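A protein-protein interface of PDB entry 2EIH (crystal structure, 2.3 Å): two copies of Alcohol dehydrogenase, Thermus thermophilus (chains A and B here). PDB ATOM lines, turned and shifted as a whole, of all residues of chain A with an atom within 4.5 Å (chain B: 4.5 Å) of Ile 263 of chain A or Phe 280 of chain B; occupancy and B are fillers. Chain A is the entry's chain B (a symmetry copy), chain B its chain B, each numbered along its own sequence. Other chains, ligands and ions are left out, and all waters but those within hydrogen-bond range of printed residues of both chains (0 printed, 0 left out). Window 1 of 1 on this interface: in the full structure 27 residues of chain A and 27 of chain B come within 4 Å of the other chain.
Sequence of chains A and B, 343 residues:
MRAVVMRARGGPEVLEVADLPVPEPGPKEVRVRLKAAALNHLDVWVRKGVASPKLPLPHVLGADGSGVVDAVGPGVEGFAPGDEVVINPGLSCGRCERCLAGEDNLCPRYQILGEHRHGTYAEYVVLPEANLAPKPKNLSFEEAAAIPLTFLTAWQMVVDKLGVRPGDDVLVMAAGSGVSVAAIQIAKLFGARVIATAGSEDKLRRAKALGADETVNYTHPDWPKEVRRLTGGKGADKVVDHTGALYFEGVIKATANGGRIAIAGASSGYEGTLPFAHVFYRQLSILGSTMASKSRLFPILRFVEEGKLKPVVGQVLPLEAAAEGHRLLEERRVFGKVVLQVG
Met 157 of chain A touches none of the printed residues of chain B.
Of the printed residues of chain B, Ile 263 of chain A touches Phe 280 (3.4 Å).
Of the printed residues of chain B, Ile 286 of chain A touches Phe 280 (3.3 Å) and Leu 284 (3.9 Å).
Of the printed residues of chain B, Gly 288 of chain A touches Phe 280, Gln 283 and Leu 284.
Val 279 of chain B touches none of the printed residues of chain A.
The nearest residue of chain A that does not touch Phe 280 of chain B is Leu 287 of chain A (4.4 Å).
The nearest printed residue of chain B that does not touch Ile 286 of chain A is Leu 274 of chain B (5.6 Å).
N of Thr 290 of chain A is in hydrogen-bond range of OE1 of Gln 283 of chain B, at 3.2 Å.
The backbone carbonyl oxygen (O) of Leu 284 of chain B is in hydrogen-bond range of the backbone NH (N) of Gly 288 of chain A (2.9 Å).
Of the 10 printed residues of chain B, 5 touch a printed residue of chain A.
Hydrophobic or aromatic side chains of chain B that line the printed part of chain A: Phe 276 and Phe 280.
Along chain B the printed residues that touch a printed residue of chain A span positions 276 to 284.
Of the 15 printed residues of chain A, 9 touch a printed residue of chain B.
Among the printed residues, 16 pairs touch across the chains.
Among the printed residues, pairs that only touch across the chains: Ile 286 of chain A with Phe 280 of chain B, Gly 244 of chain A with Phe 276 of chain B, Ile 263 of chain A with Phe 280 of chain B, Gly 265 of chain A with Phe 280 of chain B, Thr 290 of chain A with Phe 280 of chain B, Gly 288 of chain A with Phe 280 of chain B, Thr 290 of chain A with Tyr 281 of chain B, Phe 248 of chain A with Phe 276 of chain B, Gly 288 of chain A with Gln 283 of chain B, Ser 289 of chain A with Phe 280 of chain B, Ser 289 of chain A with Gln 283 of chain B, Leu 287 of chain A with Leu 284 of chain B, Ile 286 of chain A with Leu 284 of chain B and Gly 265 of chain A with Tyr 281 of chain B.
No position is printed for both chains.
N of Leu 284 of chain B is in hydrogen-bond range of O of Val 279 of chain B (2.9 Å).
The backbone carbonyl oxygen of Ile 261 of chain A lies within hydrogen-bond range of the backbone NH of Leu 287 of chain A.
OD2 of Asp 241 of chain A sits at hydrogen-bond distance from N of Gly 244 of chain A (2.8 Å).
N of Gly 265 of chain A lies within hydrogen-bond range of O of Ser 289 of chain A.
The backbone NH of Ile 263 of chain A lies within hydrogen-bond range of the backbone carbonyl oxygen of Leu 287 of chain A (2.9 Å).
O of Ile 263 of chain A lies within hydrogen-bond range of N of Ser 289 of chain A (2.9 Å).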
ATOM      1  N   MET A 157      -2.293  -1.731  -1.264  1.00  0.00           N
ATOM      2  CA  MET A 157      -2.060  -2.146  -2.647  1.00  0.00           C
ATOM      3  C   MET A 157      -0.698  -1.726  -3.187  1.00  0.00           C
ATOM      4  O   MET A 157       0.080  -2.557  -3.636  1.00  0.00           O
ATOM      5  CB  MET A 157      -3.134  -1.574  -3.573  1.00  0.00           C
ATOM      6  CG  MET A 157      -4.502  -2.012  -3.218  1.00  0.00           C
ATOM      7  SD  MET A 157      -5.641  -1.679  -4.537  1.00  0.00           S
ATOM      8  CE  MET A 157      -6.264  -0.195  -4.039  1.00  0.00           C
ATOM      9  N   ASP A 241      -5.491  -1.816  -9.902  1.00  0.00           N
ATOM     10  CA  ASP A 241      -6.794  -1.964 -10.525  1.00  0.00           C
ATOM     11  C   ASP A 241      -7.800  -1.996  -9.387  1.00  0.00           C
ATOM     12  O   ASP A 241      -7.909  -2.992  -8.677  1.00  0.00           O
ATOM     13  CB  ASP A 241      -6.825  -3.270 -11.315  1.00  0.00           C
ATOM     14  CG  ASP A 241      -8.036  -3.384 -12.217  1.00  0.00           C
ATOM     15  OD1 ASP A 241      -8.040  -4.291 -13.074  1.00  0.00           O
ATOM     16  OD2 ASP A 241      -8.984  -2.585 -12.067  1.00  0.00           O
ATOM     17  N   THR A 243     -10.746  -2.430  -9.483  1.00  0.00           N
ATOM     18  CA  THR A 243     -11.937  -3.193  -9.834  1.00  0.00           C
ATOM     19  C   THR A 243     -11.664  -4.535 -10.495  1.00  0.00           C
ATOM     20  O   THR A 243     -12.139  -5.570 -10.029  1.00  0.00           O
ATOM     21  CB  THR A 243     -12.870  -2.384 -10.762  1.00  0.00           C
ATOM     22  OG1 THR A 243     -13.838  -3.265 -11.342  1.00  0.00           O
ATOM     23  CG2 THR A 243     -12.079  -1.694 -11.875  1.00  0.00           C
ATOM     24  N   GLY A 244     -10.905  -4.516 -11.586  1.00  0.00           N
ATOM     25  CA  GLY A 244     -10.606  -5.748 -12.300  1.00  0.00           C
ATOM     26  C   GLY A 244     -11.699  -6.050 -13.316  1.00  0.00           C
ATOM     27  O   GLY A 244     -11.529  -6.879 -14.207  1.00  0.00           O
ATOM     28  N   PHE A 248      -9.973  -6.193 -18.258  1.00  0.00           N
ATOM     29  CA  PHE A 248      -8.927  -6.951 -17.598  1.00  0.00           C
ATOM     30  C   PHE A 248      -8.095  -7.732 -18.601  1.00  0.00           C
ATOM     31  O   PHE A 248      -6.961  -8.086 -18.324  1.00  0.00           O
ATOM     32  CB  PHE A 248      -9.512  -7.916 -16.567  1.00  0.00           C
ATOM     33  CG  PHE A 248      -8.522  -8.316 -15.515  1.00  0.00           C
ATOM     34  CD1 PHE A 248      -8.211  -7.442 -14.488  1.00  0.00           C
ATOM     35  CD2 PHE A 248      -7.825  -9.516 -15.607  1.00  0.00           C
ATOM     36  CE1 PHE A 248      -7.225  -7.758 -13.569  1.00  0.00           C
ATOM     37  CE2 PHE A 248      -6.832  -9.839 -14.691  1.00  0.00           C
ATOM     38  CZ  PHE A 248      -6.531  -8.962 -13.677  1.00  0.00           C
ATOM     39  N   ILE A 261      -0.255  -7.323 -10.207  1.00  0.00           N
ATOM     40  CA  ILE A 261      -1.526  -6.625 -10.396  1.00  0.00           C
ATOM     41  C   ILE A 261      -2.316  -6.738  -9.109  1.00  0.00           C
ATOM     42  O   ILE A 261      -2.617  -7.843  -8.655  1.00  0.00           O
ATOM     43  CB  ILE A 261      -2.348  -7.281 -11.507  1.00  0.00           C
ATOM     44  CG1 ILE A 261      -1.574  -7.206 -12.826  1.00  0.00           C
ATOM     45  CG2 ILE A 261      -3.704  -6.610 -11.625  1.00  0.00           C
ATOM     46  CD1 ILE A 261      -2.171  -8.057 -13.908  1.00  0.00           C
ATOM     47  N   ALA A 262      -2.639  -5.591  -8.524  1.00  0.00           N
ATOM     48  CA  ALA A 262      -3.395  -5.540  -7.283  1.00  0.00           C
ATOM     49  C   ALA A 262      -4.824  -5.143  -7.593  1.00  0.00           C
ATOM     50  O   ALA A 262      -5.065  -4.191  -8.331  1.00  0.00           O
ATOM     51  CB  ALA A 262      -2.768  -4.536  -6.324  1.00  0.00           C
ATOM     52  N   ILE A 263      -5.768  -5.886  -7.032  1.00  0.00           N
ATOM     53  CA  ILE A 263      -7.172  -5.612  -7.250  1.00  0.00           C
ATOM     54  C   ILE A 263      -7.866  -5.305  -5.938  1.00  0.00           C
ATOM     55  O   ILE A 263      -7.874  -6.118  -5.027  1.00  0.00           O
ATOM     56  CB  ILE A 263      -7.854  -6.802  -7.934  1.00  0.00           C
ATOM     57  CG1 ILE A 263      -7.165  -7.057  -9.272  1.00  0.00           C
ATOM     58  CG2 ILE A 263      -9.344  -6.535  -8.061  1.00  0.00           C
ATOM     59  CD1 ILE A 263      -7.748  -8.118 -10.109  1.00  0.00           C
ATOM     60  N   ALA A 264      -8.436  -4.111  -5.858  1.00  0.00           N
ATOM     61  CA  ALA A 264      -9.119  -3.668  -4.659  1.00  0.00           C
ATOM     62  C   ALA A 264     -10.389  -4.475  -4.460  1.00  0.00           C
ATOM     63  O   ALA A 264     -11.294  -4.446  -5.298  1.00  0.00           O
ATOM     64  CB  ALA A 264      -9.439  -2.185  -4.754  1.00  0.00           C
ATOM     65  N   GLY A 265     -10.438  -5.200  -3.342  1.00  0.00           N
ATOM     66  CA  GLY A 265     -11.585  -6.030  -3.011  1.00  0.00           C
ATOM     67  C   GLY A 265     -12.890  -5.265  -2.968  1.00  0.00           C
ATOM     68  O   GLY A 265     -12.924  -4.078  -2.640  1.00  0.00           O
ATOM     69  N   ILE A 286      -1.654 -11.891  -9.111  1.00  0.00           N
ATOM     70  CA  ILE A 286      -2.902 -11.151  -8.987  1.00  0.00           C
ATOM     71  C   ILE A 286      -3.255 -11.160  -7.514  1.00  0.00           C
ATOM     72  O   ILE A 286      -3.628 -12.196  -6.960  1.00  0.00           O
ATOM     73  CB  ILE A 286      -4.017 -11.809  -9.796  1.00  0.00           C
ATOM     74  CG1 ILE A 286      -3.622 -11.840 -11.282  1.00  0.00           C
ATOM     75  CG2 ILE A 286      -5.296 -11.024  -9.630  1.00  0.00           C
ATOM     76  CD1 ILE A 286      -4.458 -12.772 -12.093  1.00  0.00           C
ATOM     77  N   LEU A 287      -3.151  -9.997  -6.884  1.00  0.00           N
ATOM     78  CA  LEU A 287      -3.374  -9.874  -5.447  1.00  0.00           C
ATOM     79  C   LEU A 287      -4.625  -9.118  -4.979  1.00  0.00           C
ATOM     80  O   LEU A 287      -4.777  -7.923  -5.225  1.00  0.00           O
ATOM     81  CB  LEU A 287      -2.133  -9.215  -4.839  1.00  0.00           C
ATOM     82  CG  LEU A 287      -0.803  -9.821  -5.342  1.00  0.00           C
ATOM     83  CD1 LEU A 287       0.354  -8.914  -5.012  1.00  0.00           C
ATOM     84  CD2 LEU A 287      -0.629 -11.189  -4.742  1.00  0.00           C
ATOM     85  N   GLY A 288      -5.513  -9.817  -4.286  1.00  0.00           N
ATOM     86  CA  GLY A 288      -6.705  -9.171  -3.772  1.00  0.00           C
ATOM     87  C   GLY A 288      -6.276  -8.315  -2.600  1.00  0.00           C
ATOM     88  O   GLY A 288      -5.440  -8.728  -1.802  1.00  0.00           O
ATOM     89  N   SER A 289      -6.818  -7.112  -2.483  1.00  0.00           N
ATOM     90  CA  SER A 289      -6.432  -6.255  -1.373  1.00  0.00           C
ATOM     91  C   SER A 289      -7.649  -5.501  -0.867  1.00  0.00           C
ATOM     92  O   SER A 289      -8.442  -4.991  -1.653  1.00  0.00           O
ATOM     93  CB  SER A 289      -5.333  -5.286  -1.812  1.00  0.00           C
ATOM     94  OG  SER A 289      -4.801  -4.561  -0.706  1.00  0.00           O
ATOM     95  N   THR A 290      -7.804  -5.455   0.449  1.00  0.00           N
ATOM     96  CA  THR A 290      -8.938  -4.780   1.065  1.00  0.00           C
ATOM     97  C   THR A 290      -8.485  -3.988   2.289  1.00  0.00           C
ATOM     98  O   THR A 290      -7.870  -4.536   3.202  1.00  0.00           O
ATOM     99  CB  THR A 290     -10.018  -5.789   1.501  1.00  0.00           C
ATOM    100  OG1 THR A 290     -10.493  -6.492   0.350  1.00  0.00           O
ATOM    101  CG2 THR A 290     -11.178  -5.069   2.158  1.00  0.00           C
ATOM    102  N   LEU B 274     -11.443 -17.210 -13.703  1.00  0.00           N
ATOM    103  CA  LEU B 274     -10.976 -16.990 -12.331  1.00  0.00           C
ATOM    104  C   LEU B 274     -11.942 -16.078 -11.584  1.00  0.00           C
ATOM    105  O   LEU B 274     -12.174 -14.939 -11.989  1.00  0.00           O
ATOM    106  CB  LEU B 274      -9.570 -16.381 -12.326  1.00  0.00           C
ATOM    107  CG  LEU B 274      -8.905 -16.065 -10.976  1.00  0.00           C
ATOM    108  CD1 LEU B 274      -9.436 -14.759 -10.414  1.00  0.00           C
ATOM    109  CD2 LEU B 274      -9.135 -17.205 -10.003  1.00  0.00           C
ATOM    110  N   PHE B 276     -13.411 -13.386  -9.602  1.00  0.00           N
ATOM    111  CA  PHE B 276     -12.921 -12.091  -9.183  1.00  0.00           C
ATOM    112  C   PHE B 276     -13.453 -11.677  -7.836  1.00  0.00           C
ATOM    113  O   PHE B 276     -12.766 -11.779  -6.824  1.00  0.00           O
ATOM    114  CB  PHE B 276     -13.287 -11.035 -10.219  1.00  0.00           C
ATOM    115  CG  PHE B 276     -12.267 -10.880 -11.289  1.00  0.00           C
ATOM    116  CD1 PHE B 276     -11.885 -11.964 -12.060  1.00  0.00           C
ATOM    117  CD2 PHE B 276     -11.653  -9.659 -11.502  1.00  0.00           C
ATOM    118  CE1 PHE B 276     -10.904 -11.837 -13.024  1.00  0.00           C
ATOM    119  CE2 PHE B 276     -10.670  -9.523 -12.465  1.00  0.00           C
ATOM    120  CZ  PHE B 276     -10.297 -10.619 -13.228  1.00  0.00           C
ATOM    121  N   ALA B 277     -14.690 -11.204  -7.841  1.00  0.00           N
ATOM    122  CA  ALA B 277     -15.359 -10.741  -6.639  1.00  0.00           C
ATOM    123  C   ALA B 277     -14.936 -11.475  -5.376  1.00  0.00           C
ATOM    124  O   ALA B 277     -14.091 -11.004  -4.622  1.00  0.00           O
ATOM    125  CB  ALA B 277     -16.864 -10.852  -6.820  1.00  0.00           C
ATOM    126  N   HIS B 278     -15.536 -12.635  -5.154  1.00  0.00           N
ATOM    127  CA  HIS B 278     -15.256 -13.420  -3.971  1.00  0.00           C
ATOM    128  C   HIS B 278     -13.904 -14.120  -4.053  1.00  0.00           C
ATOM    129  O   HIS B 278     -13.810 -15.348  -3.977  1.00  0.00           O
ATOM    130  CB  HIS B 278     -16.379 -14.443  -3.753  1.00  0.00           C
ATOM    131  CG  HIS B 278     -16.439 -14.988  -2.359  1.00  0.00           C
ATOM    132  ND1 HIS B 278     -16.628 -14.183  -1.257  1.00  0.00           N
ATOM    133  CD2 HIS B 278     -16.352 -16.255  -1.894  1.00  0.00           C
ATOM    134  CE1 HIS B 278     -16.656 -14.934  -0.168  1.00  0.00           C
ATOM    135  NE2 HIS B 278     -16.491 -16.195  -0.528  1.00  0.00           N
ATOM    136  N   VAL B 279     -12.861 -13.322  -4.219  1.00  0.00           N
ATOM    137  CA  VAL B 279     -11.497 -13.823  -4.292  1.00  0.00           C
ATOM    138  C   VAL B 279     -10.591 -12.702  -3.852  1.00  0.00           C
ATOM    139  O   VAL B 279      -9.699 -12.885  -3.032  1.00  0.00           O
ATOM    140  CB  VAL B 279     -11.104 -14.241  -5.722  1.00  0.00           C
ATOM    141  CG1 VAL B 279      -9.605 -14.045  -5.944  1.00  0.00           C
ATOM    142  CG2 VAL B 279     -11.455 -15.701  -5.931  1.00  0.00           C
ATOM    143  N   PHE B 280     -10.831 -11.529  -4.406  1.00  0.00           N
ATOM    144  CA  PHE B 280     -10.038 -10.388  -4.046  1.00  0.00           C
ATOM    145  C   PHE B 280     -10.643  -9.752  -2.810  1.00  0.00           C
ATOM    146  O   PHE B 280      -9.977  -9.013  -2.090  1.00  0.00           O
ATOM    147  CB  PHE B 280      -9.989  -9.426  -5.221  1.00  0.00           C
ATOM    148  CG  PHE B 280      -9.515 -10.069  -6.489  1.00  0.00           C
ATOM    149  CD1 PHE B 280      -8.343 -10.822  -6.502  1.00  0.00           C
ATOM    150  CD2 PHE B 280     -10.235  -9.923  -7.669  1.00  0.00           C
ATOM    151  CE1 PHE B 280      -7.894 -11.422  -7.677  1.00  0.00           C
ATOM    152  CE2 PHE B 280      -9.798 -10.516  -8.850  1.00  0.00           C
ATOM    153  CZ  PHE B 280      -8.625 -11.267  -8.855  1.00  0.00           C
ATOM    154  N   TYR B 281     -11.910 -10.054  -2.558  1.00  0.00           N
ATOM    155  CA  TYR B 281     -12.575  -9.521  -1.385  1.00  0.00           C
ATOM    156  C   TYR B 281     -12.055 -10.275  -0.174  1.00  0.00           C
ATOM    157  O   TYR B 281     -11.967  -9.727   0.923  1.00  0.00           O
ATOM    158  CB  TYR B 281     -14.085  -9.704  -1.475  1.00  0.00           C
ATOM    159  CG  TYR B 281     -14.831  -9.007  -0.362  1.00  0.00           C
ATOM    160  CD1 TYR B 281     -14.612  -7.651  -0.092  1.00  0.00           C
ATOM    161  CD2 TYR B 281     -15.776  -9.686   0.404  1.00  0.00           C
ATOM    162  CE1 TYR B 281     -15.320  -6.985   0.910  1.00  0.00           C
ATOM    163  CE2 TYR B 281     -16.493  -9.030   1.406  1.00  0.00           C
ATOM    164  CZ  TYR B 281     -16.261  -7.680   1.652  1.00  0.00           C
ATOM    165  OH  TYR B 281     -16.986  -7.017   2.616  1.00  0.00           O
ATOM    166  N   ARG B 282     -11.720 -11.546  -0.374  1.00  0.00           N
ATOM    167  CA  ARG B 282     -11.189 -12.361   0.708  1.00  0.00           C
ATOM    168  C   ARG B 282      -9.678 -12.220   0.744  1.00  0.00           C
ATOM    169  O   ARG B 282      -8.991 -12.943   1.454  1.00  0.00           O
ATOM    170  CB  ARG B 282     -11.572 -13.816   0.506  1.00  0.00           C
ATOM    171  CG  ARG B 282     -13.053 -14.041   0.546  1.00  0.00           C
ATOM    172  CD  ARG B 282     -13.337 -15.472   0.237  1.00  0.00           C
ATOM    173  NE  ARG B 282     -12.675 -16.336   1.190  1.00  0.00           N
ATOM    174  CZ  ARG B 282     -12.387 -17.609   0.962  1.00  0.00           C
ATOM    175  NH1 ARG B 282     -12.700 -18.167  -0.199  1.00  0.00           N
ATOM    176  NH2 ARG B 282     -11.795 -18.321   1.908  1.00  0.00           N
ATOM    177  N   GLN B 283      -9.185 -11.279  -0.045  1.00  0.00           N
ATOM    178  CA  GLN B 283      -7.772 -10.985  -0.118  1.00  0.00           C
ATOM    179  C   GLN B 283      -6.897 -12.168  -0.456  1.00  0.00           C
ATOM    180  O   GLN B 283      -5.872 -12.398   0.174  1.00  0.00           O
ATOM    181  CB  GLN B 283      -7.301 -10.346   1.190  1.00  0.00           C
ATOM    182  CG  GLN B 283      -8.034  -9.058   1.485  1.00  0.00           C
ATOM    183  CD  GLN B 283      -7.346  -8.241   2.533  1.00  0.00           C
ATOM    184  OE1 GLN B 283      -6.306  -7.636   2.273  1.00  0.00           O
ATOM    185  NE2 GLN B 283      -7.907  -8.226   3.740  1.00  0.00           N
ATOM    186  N   LEU B 284      -7.305 -12.911  -1.469  1.00  0.00           N
ATOM    187  CA  LEU B 284      -6.568 -14.073  -1.924  1.00  0.00           C
ATOM    188  C   LEU B 284      -5.486 -13.638  -2.917  1.00  0.00           C
ATOM    189  O   LEU B 284      -5.637 -12.642  -3.631  1.00  0.00           O
ATOM    190  CB  LEU B 284      -7.539 -15.056  -2.588  1.00  0.00           C
ATOM    191  CG  LEU B 284      -8.150 -16.186  -1.737  1.00  0.00           C
ATOM    192  CD1 LEU B 284      -8.310 -15.758  -0.293  1.00  0.00           C
ATOM    193  CD2 LEU B 284      -9.496 -16.611  -2.335  1.00  0.00           C
